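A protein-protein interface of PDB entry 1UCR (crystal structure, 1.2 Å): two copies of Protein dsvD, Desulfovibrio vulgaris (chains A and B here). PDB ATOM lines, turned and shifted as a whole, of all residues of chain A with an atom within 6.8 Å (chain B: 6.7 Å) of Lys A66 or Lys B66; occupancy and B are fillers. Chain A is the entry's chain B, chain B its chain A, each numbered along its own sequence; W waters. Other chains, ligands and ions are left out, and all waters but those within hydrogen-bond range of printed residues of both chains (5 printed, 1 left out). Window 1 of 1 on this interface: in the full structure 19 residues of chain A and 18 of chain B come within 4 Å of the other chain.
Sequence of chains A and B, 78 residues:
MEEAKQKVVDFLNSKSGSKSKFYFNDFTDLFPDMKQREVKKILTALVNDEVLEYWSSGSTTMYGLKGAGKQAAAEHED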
ATOM      1  N   GLN A   6      18.770  -7.706  34.718  1.00  0.00           N
ATOM      2  CA  GLN A   6      20.131  -7.578  34.297  1.00  0.00           C
ATOM      3  C   GLN A   6      20.784  -8.950  34.095  1.00  0.00           C
ATOM      4  O   GLN A   6      21.579  -9.150  33.165  1.00  0.00           O
ATOM      5  CB  GLN A   6      20.955  -6.757  35.323  1.00  0.00           C
ATOM      6  CG  GLN A   6      22.382  -6.495  34.801  1.00  0.00           C
ATOM      7  CD  GLN A   6      22.245  -5.548  33.613  1.00  0.00           C
ATOM      8  OE1 GLN A   6      21.753  -4.434  33.745  1.00  0.00           O
ATOM      9  NE2 GLN A   6      22.677  -5.942  32.429  1.00  0.00           N
ATOM     10  N   VAL A   9      19.745 -10.180  30.666  1.00  0.00           N
ATOM     11  CA  VAL A   9      20.496  -9.498  29.621  1.00  0.00           C
ATOM     12  C   VAL A   9      21.949 -10.000  29.580  1.00  0.00           C
ATOM     13  O   VAL A   9      22.527 -10.253  28.506  1.00  0.00           O
ATOM     14  CB  VAL A   9      20.456  -7.992  29.835  1.00  0.00           C
ATOM     15  CG1 VAL A   9      21.363  -7.219  28.895  1.00  0.00           C
ATOM     16  CG2 VAL A   9      19.013  -7.518  29.634  1.00  0.00           C
ATOM     17  N   ASP A  10      22.568 -10.127  30.781  1.00  0.00           N
ATOM     18  CA  ASP A  10      23.983 -10.548  30.791  1.00  0.00           C
ATOM     19  C   ASP A  10      24.159 -11.955  30.221  1.00  0.00           C
ATOM     20  O   ASP A  10      25.136 -12.228  29.516  1.00  0.00           O
ATOM     21  CB  ASP A  10      24.544 -10.563  32.210  1.00  0.00           C
ATOM     22  CG  ASP A  10      24.715  -9.155  32.820  1.00  0.00           C
ATOM     23  OD1 ASP A  10      24.560  -8.161  32.079  1.00  0.00           O
ATOM     24  OD2 ASP A  10      24.960  -9.084  34.029  1.00  0.00           O
ATOM     25  N   ASN A  13      23.827 -11.556  26.381  1.00  0.00           N
ATOM     26  CA  ASN A  13      24.855 -10.713  25.786  1.00  0.00           C
ATOM     27  C   ASN A  13      26.206 -11.370  25.981  1.00  0.00           C
ATOM     28  O   ASN A  13      27.086 -10.878  26.637  1.00  0.00           O
ATOM     29  CB  ASN A  13      24.776  -9.332  26.426  1.00  0.00           C
ATOM     30  CG  ASN A  13      25.662  -8.313  25.734  1.00  0.00           C
ATOM     31  OD1 ASN A  13      25.884  -8.386  24.539  1.00  0.00           O
ATOM     32  ND2 ASN A  13      26.135  -7.353  26.520  1.00  0.00           N
ATOM     33  N   VAL A  47      10.449  -7.612  27.012  1.00  0.00           N
ATOM     34  CA  VAL A  47       9.914  -7.488  25.626  1.00  0.00           C
ATOM     35  C   VAL A  47       9.161  -6.197  25.495  1.00  0.00           C
ATOM     36  O   VAL A  47       9.335  -5.492  24.467  1.00  0.00           O
ATOM     37  CB  VAL A  47       9.029  -8.724  25.327  1.00  0.00           C
ATOM     38  CG1 VAL A  47       8.300  -8.489  24.018  1.00  0.00           C
ATOM     39  CG2 VAL A  47       9.858  -9.991  25.281  1.00  0.00           C
ATOM     40  N   GLU A  50      11.418  -3.461  24.846  1.00  0.00           N
ATOM     41  CA  GLU A  50      12.142  -3.687  23.612  1.00  0.00           C
ATOM     42  C   GLU A  50      13.613  -3.967  23.881  1.00  0.00           C
ATOM     43  O   GLU A  50      14.441  -3.853  22.966  1.00  0.00           O
ATOM     44  CB  GLU A  50      11.972  -2.558  22.592  1.00  0.00           C
ATOM     45  CG  GLU A  50      10.493  -2.411  22.225  1.00  0.00           C
ATOM     46  CD  GLU A  50      10.251  -1.407  21.179  1.00  0.00           C
ATOM     47  OE1 GLU A  50       9.410  -0.495  21.372  1.00  0.00           O
ATOM     48  OE2 GLU A  50      10.892  -1.500  20.109  1.00  0.00           O
ATOM     49  N   VAL A  51      13.949  -4.411  25.086  1.00  0.00           N
ATOM     50  CA  VAL A  51      15.259  -4.995  25.346  1.00  0.00           C
ATOM     51  C   VAL A  51      15.327  -6.387  24.736  1.00  0.00           C
ATOM     52  O   VAL A  51      16.348  -6.802  24.227  1.00  0.00           O
ATOM     53  CB  VAL A  51      15.527  -5.052  26.859  1.00  0.00           C
ATOM     54  CG1 VAL A  51      16.843  -5.749  27.175  1.00  0.00           C
ATOM     55  CG2 VAL A  51      15.522  -3.640  27.411  1.00  0.00           C
ATOM     56  N   LEU A  52      14.202  -7.119  24.818  1.00  0.00           N
ATOM     57  CA  LEU A  52      14.096  -8.426  24.204  1.00  0.00           C
ATOM     58  C   LEU A  52      13.092  -8.409  23.071  1.00  0.00           C
ATOM     59  O   LEU A  52      12.223  -7.524  22.993  1.00  0.00           O
ATOM     60  CB  LEU A  52      13.595  -9.510  25.203  1.00  0.00           C
ATOM     61  CG  LEU A  52      14.492  -9.706  26.418  1.00  0.00           C
ATOM     62  CD1 LEU A  52      13.897 -10.763  27.343  1.00  0.00           C
ATOM     63  CD2 LEU A  52      15.907 -10.066  26.043  1.00  0.00           C
ATOM     64  N   GLU A  53      13.208  -9.407  22.202  1.00  0.00           N
ATOM     65  CA  GLU A  53      12.191  -9.758  21.204  1.00  0.00           C
ATOM     66  C   GLU A  53      11.674 -11.152  21.523  1.00  0.00           C
ATOM     67  O   GLU A  53      12.370 -11.985  22.120  1.00  0.00           O
ATOM     68  CB  GLU A  53      12.759  -9.597  19.822  1.00  0.00           C
ATOM     69  CG  GLU A  53      13.965 -10.421  19.526  1.00  0.00           C
ATOM     70  CD  GLU A  53      14.701 -10.029  18.288  1.00  0.00           C
ATOM     71  OE1 GLU A  53      15.497 -10.907  17.822  1.00  0.00           O
ATOM     72  OE2 GLU A  53      14.579  -8.900  17.767  1.00  0.00           O
ATOM     73  N   TYR A  54      10.422 -11.354  21.103  1.00  0.00           N
ATOM     74  CA  TYR A  54       9.639 -12.537  21.465  1.00  0.00           C
ATOM     75  C   TYR A  54       9.260 -13.369  20.270  1.00  0.00           C
ATOM     76  O   TYR A  54       8.956 -12.807  19.192  1.00  0.00           O
ATOM     77  CB  TYR A  54       8.364 -12.053  22.076  1.00  0.00           C
ATOM     78  CG  TYR A  54       7.282 -12.997  22.476  1.00  0.00           C
ATOM     79  CD1 TYR A  54       6.182 -13.231  21.661  1.00  0.00           C
ATOM     80  CD2 TYR A  54       7.349 -13.658  23.713  1.00  0.00           C
ATOM     81  CE1 TYR A  54       5.160 -14.113  22.046  1.00  0.00           C
ATOM     82  CE2 TYR A  54       6.306 -14.487  24.099  1.00  0.00           C
ATOM     83  CZ  TYR A  54       5.247 -14.711  23.290  1.00  0.00           C
ATOM     84  OH  TYR A  54       4.212 -15.544  23.682  1.00  0.00           O
ATOM     85  N   GLY A  64      15.061 -13.402  22.804  1.00  0.00           N
ATOM     86  CA  GLY A  64      16.443 -12.993  22.575  1.00  0.00           C
ATOM     87  C   GLY A  64      16.556 -11.486  22.629  1.00  0.00           C
ATOM     88  O   GLY A  64      15.559 -10.779  22.738  1.00  0.00           O
ATOM     89  N   LEU A  65      17.811 -10.991  22.612  1.00  0.00           N
ATOM     90  CA  LEU A  65      17.968  -9.544  22.631  1.00  0.00           C
ATOM     91  C   LEU A  65      17.441  -8.880  21.359  1.00  0.00           C
ATOM     92  O   LEU A  65      17.530  -9.436  20.267  1.00  0.00           O
ATOM     93  CB  LEU A  65      19.497  -9.229  22.763  1.00  0.00           C
ATOM     94  CG  LEU A  65      20.016  -9.523  24.167  1.00  0.00           C
ATOM     95  CD1 LEU A  65      21.548  -9.565  24.160  1.00  0.00           C
ATOM     96  CD2 LEU A  65      19.529  -8.533  25.249  1.00  0.00           C
ATOM     97  N   LYS A  66      16.843  -7.681  21.489  1.00  0.00           N
ATOM     98  CA  LYS A  66      16.269  -6.979  20.340  1.00  0.00           C
ATOM     99  C   LYS A  66      17.283  -6.857  19.239  1.00  0.00           C
ATOM    100  O   LYS A  66      18.410  -6.393  19.490  1.00  0.00           O
ATOM    101  CB  LYS A  66      15.858  -5.583  20.815  1.00  0.00           C
ATOM    102  CG  LYS A  66      15.045  -4.815  19.804  1.00  0.00           C
ATOM    103  CD  LYS A  66      13.640  -5.427  19.681  1.00  0.00           C
ATOM    104  CE  LYS A  66      12.700  -4.512  18.881  1.00  0.00           C
ATOM    105  NZ  LYS A  66      11.435  -5.311  18.634  1.00  0.00           N
ATOM    106  N   GLY A  67      16.882  -7.221  18.050  1.00  0.00           N
ATOM    107  CA  GLY A  67      17.770  -7.152  16.885  1.00  0.00           C
ATOM    108  C   GLY A  67      18.460  -8.457  16.585  1.00  0.00           C
ATOM    109  O   GLY A  67      18.969  -8.637  15.457  1.00  0.00           O
ATOM    110  N   ALA A  68      18.525  -9.419  17.506  1.00  0.00           N
ATOM    111  CA  ALA A  68      19.271 -10.650  17.265  1.00  0.00           C
ATOM    112  C   ALA A  68      18.711 -11.447  16.116  1.00  0.00           C
ATOM    113  O   ALA A  68      19.539 -12.048  15.361  1.00  0.00           O
ATOM    114  CB  ALA A  68      19.277 -11.510  18.535  1.00  0.00           C
ATOM    115  N   GLY A  69      17.377 -11.465  15.998  1.00  0.00           N
ATOM    116  CA  GLY A  69      16.764 -12.218  14.883  1.00  0.00           C
ATOM    117  C   GLY A  69      17.184 -11.729  13.525  1.00  0.00           C
ATOM    118  O   GLY A  69      17.579 -12.478  12.579  1.00  0.00           O
ATOM    119  N   GLN B   6      11.666   4.993  19.173  1.00  0.00           N
ATOM    120  CA  GLN B   6      11.211   3.880  18.343  1.00  0.00           C
ATOM    121  C   GLN B   6      11.767   3.967  16.930  1.00  0.00           C
ATOM    122  O   GLN B   6      12.050   2.965  16.294  1.00  0.00           O
ATOM    123  CB  GLN B   6       9.688   3.870  18.251  1.00  0.00           C
ATOM    124  CG  GLN B   6       9.137   2.573  17.651  1.00  0.00           C
ATOM    125  CD  GLN B   6       9.413   1.354  18.479  1.00  0.00           C
ATOM    126  OE1 GLN B   6       8.903   1.263  19.595  1.00  0.00           O
ATOM    127  NE2 GLN B   6      10.245   0.451  17.987  1.00  0.00           N
ATOM    128  N   VAL B   9      15.248   2.526  17.101  1.00  0.00           N
ATOM    129  CA  VAL B   9      15.205   1.053  17.193  1.00  0.00           C
ATOM    130  C   VAL B   9      14.804   0.444  15.871  1.00  0.00           C
ATOM    131  O   VAL B   9      15.430  -0.514  15.396  1.00  0.00           O
ATOM    132  CB  VAL B   9      14.227   0.642  18.294  1.00  0.00           C
ATOM    133  CG1 VAL B   9      13.995  -0.865  18.230  1.00  0.00           C
ATOM    134  CG2 VAL B   9      14.784   1.066  19.647  1.00  0.00           C
ATOM    135  N   ASP B  10      13.774   1.025  15.218  1.00  0.00           N
ATOM    136  CA  ASP B  10      13.343   0.427  13.960  1.00  0.00           C
ATOM    137  C   ASP B  10      14.418   0.538  12.891  1.00  0.00           C
ATOM    138  O   ASP B  10      14.539  -0.360  12.013  1.00  0.00           O
ATOM    139  CB  ASP B  10      12.081   1.154  13.492  1.00  0.00           C
ATOM    140  CG  ASP B  10      10.870   0.874  14.340  1.00  0.00           C
ATOM    141  OD1 ASP B  10      10.874  -0.039  15.185  1.00  0.00           O
ATOM    142  OD2 ASP B  10       9.834   1.575  14.146  1.00  0.00           O
ATOM    143  N   ASN B  13      16.901  -2.231  13.644  1.00  0.00           N
ATOM    144  CA  ASN B  13      16.346  -3.586  13.703  1.00  0.00           C
ATOM    145  C   ASN B  13      15.972  -3.994  12.281  1.00  0.00           C
ATOM    146  O   ASN B  13      14.788  -4.076  11.896  1.00  0.00           O
ATOM    147  CB  ASN B  13      15.148  -3.617  14.629  1.00  0.00           C
ATOM    148  CG  ASN B  13      14.569  -5.000  14.903  1.00  0.00           C
ATOM    149  OD1 ASN B  13      13.372  -5.117  15.264  1.00  0.00           O
ATOM    150  ND2 ASN B  13      15.404  -5.982  14.764  1.00  0.00           N
ATOM    151  N   VAL B  47      20.559   3.510  25.685  1.00  0.00           N
ATOM    152  CA  VAL B  47      21.664   2.764  26.271  1.00  0.00           C
ATOM    153  C   VAL B  47      21.383   2.478  27.747  1.00  0.00           C
ATOM    154  O   VAL B  47      21.564   1.349  28.219  1.00  0.00           O
ATOM    155  CB  VAL B  47      22.995   3.550  26.092  1.00  0.00           C
ATOM    156  CG1 VAL B  47      24.109   2.955  26.941  1.00  0.00           C
ATOM    157  CG2 VAL B  47      23.424   3.608  24.626  1.00  0.00           C
ATOM    158  N   GLU B  50      19.203  -0.299  28.081  1.00  0.00           N
ATOM    159  CA  GLU B  50      19.831  -1.487  27.542  1.00  0.00           C
ATOM    160  C   GLU B  50      19.127  -2.020  26.310  1.00  0.00           C
ATOM    161  O   GLU B  50      19.316  -3.182  25.934  1.00  0.00           O
ATOM    162  CB  GLU B  50      20.055  -2.601  28.610  1.00  0.00           C
ATOM    163  CG  GLU B  50      20.934  -1.987  29.714  1.00  0.00           C
ATOM    164  CD  GLU B  50      21.385  -3.020  30.687  1.00  0.00           C
ATOM    165  OE1 GLU B  50      21.957  -4.070  30.335  1.00  0.00           O
ATOM    166  OE2 GLU B  50      21.203  -2.749  31.902  1.00  0.00           O
ATOM    167  N   VAL B  51      18.385  -1.163  25.622  1.00  0.00           N
ATOM    168  CA  VAL B  51      17.951  -1.442  24.258  1.00  0.00           C
ATOM    169  C   VAL B  51      19.117  -1.303  23.277  1.00  0.00           C
ATOM    170  O   VAL B  51      19.269  -2.094  22.360  1.00  0.00           O
ATOM    171  CB  VAL B  51      16.788  -0.513  23.883  1.00  0.00           C
ATOM    172  CG1 VAL B  51      16.350  -0.745  22.446  1.00  0.00           C
ATOM    173  CG2 VAL B  51      15.590  -0.712  24.836  1.00  0.00           C
ATOM    174  N   LEU B  52      19.923  -0.263  23.512  1.00  0.00           N
ATOM    175  CA  LEU B  52      21.162  -0.057  22.724  1.00  0.00           C
ATOM    176  C   LEU B  52      22.370  -0.349  23.614  1.00  0.00           C
ATOM    177  O   LEU B  52      22.287  -0.340  24.837  1.00  0.00           O
ATOM    178  CB  LEU B  52      21.322   1.366  22.249  1.00  0.00           C
ATOM    179  CG  LEU B  52      20.316   1.873  21.244  1.00  0.00           C
ATOM    180  CD1 LEU B  52      20.566   3.356  20.864  1.00  0.00           C
ATOM    181  CD2 LEU B  52      20.237   1.017  20.015  1.00  0.00           C
ATOM    182  N   GLU B  53      23.476  -0.583  22.898  1.00  0.00           N
ATOM    183  CA  GLU B  53      24.824  -0.524  23.491  1.00  0.00           C
ATOM    184  C   GLU B  53      25.625   0.499  22.691  1.00  0.00           C
ATOM    185  O   GLU B  53      25.283   0.829  21.553  1.00  0.00           O
ATOM    186  CB  GLU B  53      25.543  -1.876  23.387  1.00  0.00           C
ATOM    187  CG  GLU B  53      25.702  -2.317  21.953  1.00  0.00           C
ATOM    188  CD  GLU B  53      26.097  -3.772  21.818  1.00  0.00           C
ATOM    189  OE1 GLU B  53      26.544  -4.120  20.709  1.00  0.00           O
ATOM    190  OE2 GLU B  53      25.935  -4.592  22.766  1.00  0.00           O
ATOM    191  N   TYR B  54      26.650   1.055  23.311  1.00  0.00           N
ATOM    192  CA  TYR B  54      27.466   2.009  22.559  1.00  0.00           C
ATOM    193  C   TYR B  54      28.882   1.952  23.099  1.00  0.00           C
ATOM    194  O   TYR B  54      29.120   1.478  24.216  1.00  0.00           O
ATOM    195  CB  TYR B  54      26.930   3.436  22.576  1.00  0.00           C
ATOM    196  CG  TYR B  54      27.371   4.384  23.671  1.00  0.00           C
ATOM    197  CD1 TYR B  54      27.236   4.112  25.019  1.00  0.00           C
ATOM    198  CD2 TYR B  54      27.919   5.624  23.312  1.00  0.00           C
ATOM    199  CE1 TYR B  54      27.635   5.010  25.999  1.00  0.00           C
ATOM    200  CE2 TYR B  54      28.309   6.560  24.267  1.00  0.00           C
ATOM    201  CZ  TYR B  54      28.170   6.242  25.606  1.00  0.00           C
ATOM    202  OH  TYR B  54      28.537   7.159  26.565  1.00  0.00           O
ATOM    203  N   GLY B  64      24.638   0.439  18.633  1.00  0.00           N
ATOM    204  CA  GLY B  64      23.939  -0.673  18.008  1.00  0.00           C
ATOM    205  C   GLY B  64      22.903  -1.211  18.972  1.00  0.00           C
ATOM    206  O   GLY B  64      22.905  -0.911  20.160  1.00  0.00           O
ATOM    207  N   LEU B  65      22.043  -2.090  18.441  1.00  0.00           N
ATOM    208  CA  LEU B  65      21.146  -2.803  19.380  1.00  0.00           C
ATOM    209  C   LEU B  65      21.955  -3.682  20.305  1.00  0.00           C
ATOM    210  O   LEU B  65      22.949  -4.290  19.911  1.00  0.00           O
ATOM    211  CB  LEU B  65      20.131  -3.594  18.558  1.00  0.00           C
ATOM    212  CG  LEU B  65      19.068  -2.690  17.886  1.00  0.00           C
ATOM    213  CD1 LEU B  65      18.329  -3.482  16.813  1.00  0.00           C
ATOM    214  CD2 LEU B  65      18.107  -2.134  18.911  1.00  0.00           C
ATOM    215  N   LYS B  66      21.496  -3.786  21.564  1.00  0.00           N
ATOM    216  CA  LYS B  66      22.214  -4.523  22.633  1.00  0.00           C
ATOM    217  C   LYS B  66      22.464  -5.921  22.108  1.00  0.00           C
ATOM    218  O   LYS B  66      21.577  -6.594  21.606  1.00  0.00           O
ATOM    219  CB  LYS B  66      21.365  -4.547  23.888  1.00  0.00           C
ATOM    220  CG  LYS B  66      21.923  -5.198  25.171  1.00  0.00           C
ATOM    221  CD  LYS B  66      22.784  -4.232  25.891  1.00  0.00           C
ATOM    222  CE  LYS B  66      23.504  -4.723  27.140  1.00  0.00           C
ATOM    223  NZ  LYS B  66      24.711  -3.878  27.326  1.00  0.00           N
ATOM    224  N   GLY B  67      23.676  -6.432  22.311  1.00  0.00           N
ATOM    225  CA  GLY B  67      24.068  -7.742  21.919  1.00  0.00           C
ATOM    226  C   GLY B  67      24.710  -7.817  20.559  1.00  0.00           C
ATOM    227  O   GLY B  67      25.308  -8.815  20.213  1.00  0.00           O
ATOM    228  N   ALA B  68      24.593  -6.737  19.773  1.00  0.00           N
ATOM    229  CA  ALA B  68      25.044  -6.827  18.389  1.00  0.00           C
ATOM    230  C   ALA B  68      26.539  -7.086  18.323  1.00  0.00           C
ATOM    231  O   ALA B  68      27.014  -7.883  17.490  1.00  0.00           O
ATOM    232  CB  ALA B  68      24.658  -5.519  17.716  1.00  0.00           C
ATOM    233  N   GLY B  69      27.311  -6.434  19.198  1.00  0.00           N
ATOM    234  CA  GLY B  69      28.757  -6.562  19.245  1.00  0.00           C
ATOM    235  C   GLY B  69      29.203  -7.969  19.494  1.00  0.00           C
ATOM    236  O   GLY B  69      30.069  -8.560  18.825  1.00  0.00           O
ATOM    237  N   GLN B  71      27.254 -10.744  19.186  1.00  0.00           N
ATOM    238  CA  GLN B  71      26.711 -11.690  18.193  1.00  0.00           C
ATOM    239  C   GLN B  71      27.678 -11.803  17.008  1.00  0.00           C
ATOM    240  O   GLN B  71      28.083 -12.840  16.502  1.00  0.00           O
ATOM    241  CB  GLN B  71      25.416 -11.196  17.603  1.00  0.00           C
ATOM    242  CG  GLN B  71      24.064 -11.365  18.138  1.00  0.00           C
ATOM    243  CD  GLN B  71      22.902 -11.960  17.406  1.00  0.00           C
ATOM    244  OE1 GLN B  71      21.948 -12.233  18.158  1.00  0.00           O
ATOM    245  NE2 GLN B  71      22.726 -12.268  16.134  1.00  0.00           N
HETATM  246  O   HOH W   1      27.368  -6.987  22.623  1.00  0.00           O
HETATM  247  O   HOH W   2      26.620  -4.543  25.314  1.00  0.00           O
HETATM  248  O   HOH W   3      12.417  -7.403  16.985  1.00  0.00           O
HETATM  249  O   HOH W   4      15.440  -8.830  15.125  1.00  0.00           O
HETATM  250  O   HOH W   5      18.792  -5.566  24.238  1.00  0.00           O
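Asn A13 touches Gly B67, and with the chains exchanged Gly A67 touches Asn B13.
Val A51 touches its own counterpart, Val B51.
Leu A65 touches Lys B66, and with the chains exchanged Lys A66 touches Leu B65.
Lys A66 touches its own counterpart, Lys B66.
Positions printed for both chains: 6, 9, 10, 13, 47, 50, 51, 52, 53, 54, 64, 65, 66, 67, 68 and 69.
Of the 19 pairs that touch across the chains among the printed residues, 18 have their exchanged pair printed and touching as well.
Water W2 lies within hydrogen-bond range of the side-chain carboxylate (OE2) of Glu B53 (2.6 Å), the side-chain amino group (NZ) of Lys B66 (2.9 Å) and the side-chain amide nitrogen (ND2) of Asn A13 (3.1 Å).
Water W5 lies within hydrogen-bond range of O of Val A51 and O of Glu B50.
Water W3 lies within hydrogen-bond range of the side-chain carboxylate (OE2) of Glu A53 (2.7 Å), the side-chain amino group (NZ) of Lys A66 (2.8 Å) and the side-chain amide oxygen (OD1) of Asn B13 (3.0 Å).
Water W4 lies within hydrogen-bond range of OE2 of Glu A53 (2.8 Å), ND2 of Asn B13 (2.9 Å) and N of Gly A69 (3.4 Å).
Water W1 lies within hydrogen-bond range of the side-chain carboxylate of Glu B53 (2.8 Å), the side-chain amide oxygen of Asn A13 (2.8 Å) and the backbone NH of Gly B69 (3.5 Å).
Of the 16 printed residues of chain A, 9 touch a printed residue of chain B.
Hydrophobic or aromatic side chains of chain A within 4 Å of the printed part of chain B: Val A9, Val A51, Leu A65 and Ala A68.
Along chain A the printed residues that touch a printed residue of chain B span positions 6 to 68.
Among the printed residues, no Asp or Glu carboxylate lies within 4 Å of a Lys or Arg side-chain nitrogen of the other chain.
The backbone NH (N) of Gly B67 sits at hydrogen-bond distance from the side-chain carboxylate (OE2) of Glu B53, at 2.9 Å.
The backbone carbonyl oxygen (O) of Val A51 lies within hydrogen-bond range of the backbone NH (N) of Lys A66 (2.9 Å).
The backbone NH (N) of Gly A67 lies within hydrogen-bond range of the side-chain carboxylate (OE2) of Glu A53 (2.9 Å).
The side-chain carboxylate (OD1) of Asp B10 sits at hydrogen-bond distance from the side-chain amide nitrogen (NE2) of Gln B6, at 2.9 Å.
The side-chain amide nitrogen (NE2) of Gln A6 is in hydrogen-bond range of the side-chain carboxylate (OD1) of Asp A10, 2.9 Å away.
N of Lys B66 is in hydrogen-bond range of O of Val B51, 2.9 Å away.
Among the printed residues, merely in contact across the chains: Val A9 with Glu B50 (3.5 Å), Val A9 with Lys B66 (3.7 Å), Asn A13 with Lys B66 (3.8 Å), Asn A13 with Gly B67 (3.3 Å), Glu A50 with Val B9 (3.7 Å), Glu A50 with Val B51 (3.7 Å), Val A51 with Glu B50 (3.8 Å), Val A51 with Val B51 (3.9 Å), Leu A65 with Lys B66 (3.6 Å), Leu A65 with Gly B67 (3.8 Å), Lys A66 with Val B9 (3.9 Å), Lys A66 with Asn B13 (3.7 Å), Lys A66 with Leu B65 (3.4 Å), Lys A66 with Lys B66 (3.8 Å), Gly A67 with Asn B13 (3.4 Å) and Gly A67 with Leu B65 (3.7 Å).
Of the printed residues of chain B, Gln A6 touches Glu B50 (2.6 Å).
Of the printed residues of chain B, Val A9 touches Glu B50 and Lys B66.
Tyr A54 touches none of the printed residues of chain B.
Of chain B, only Val B9, Asn B13, Leu B65 and Lys B66 come within 4 Å of Lys A66.
Of the printed residues of chain A, Gln B6 touches Glu A50.
Printed residues of chain A within 4 Å of Lys B66: Val A9 (3.7 Å), Asn A13 (3.8 Å), Leu A65 (3.6 Å) and Lys A66 (3.8 Å).
The nearest residue of chain B that does not touch Lys A66 is Val B51 (5.0 Å).
The nearest printed residue of chain A that does not touch Lys B66 is Val A51 (5.5 Å).
The side-chain amide oxygen (OE1) of Gln A6 sits close to the side-chain carboxylate (OE2) of Glu B50 (2.6 Å).
The backbone carbonyl oxygen (O) of Ala A68 lies within hydrogen-bond range of the side-chain amide nitrogen (NE2) of Gln B71 (3.3 Å).
The side-chain amide oxygen of Gln B6 lies close to the side-chain carboxylate of Glu A50 (2.6 Å).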
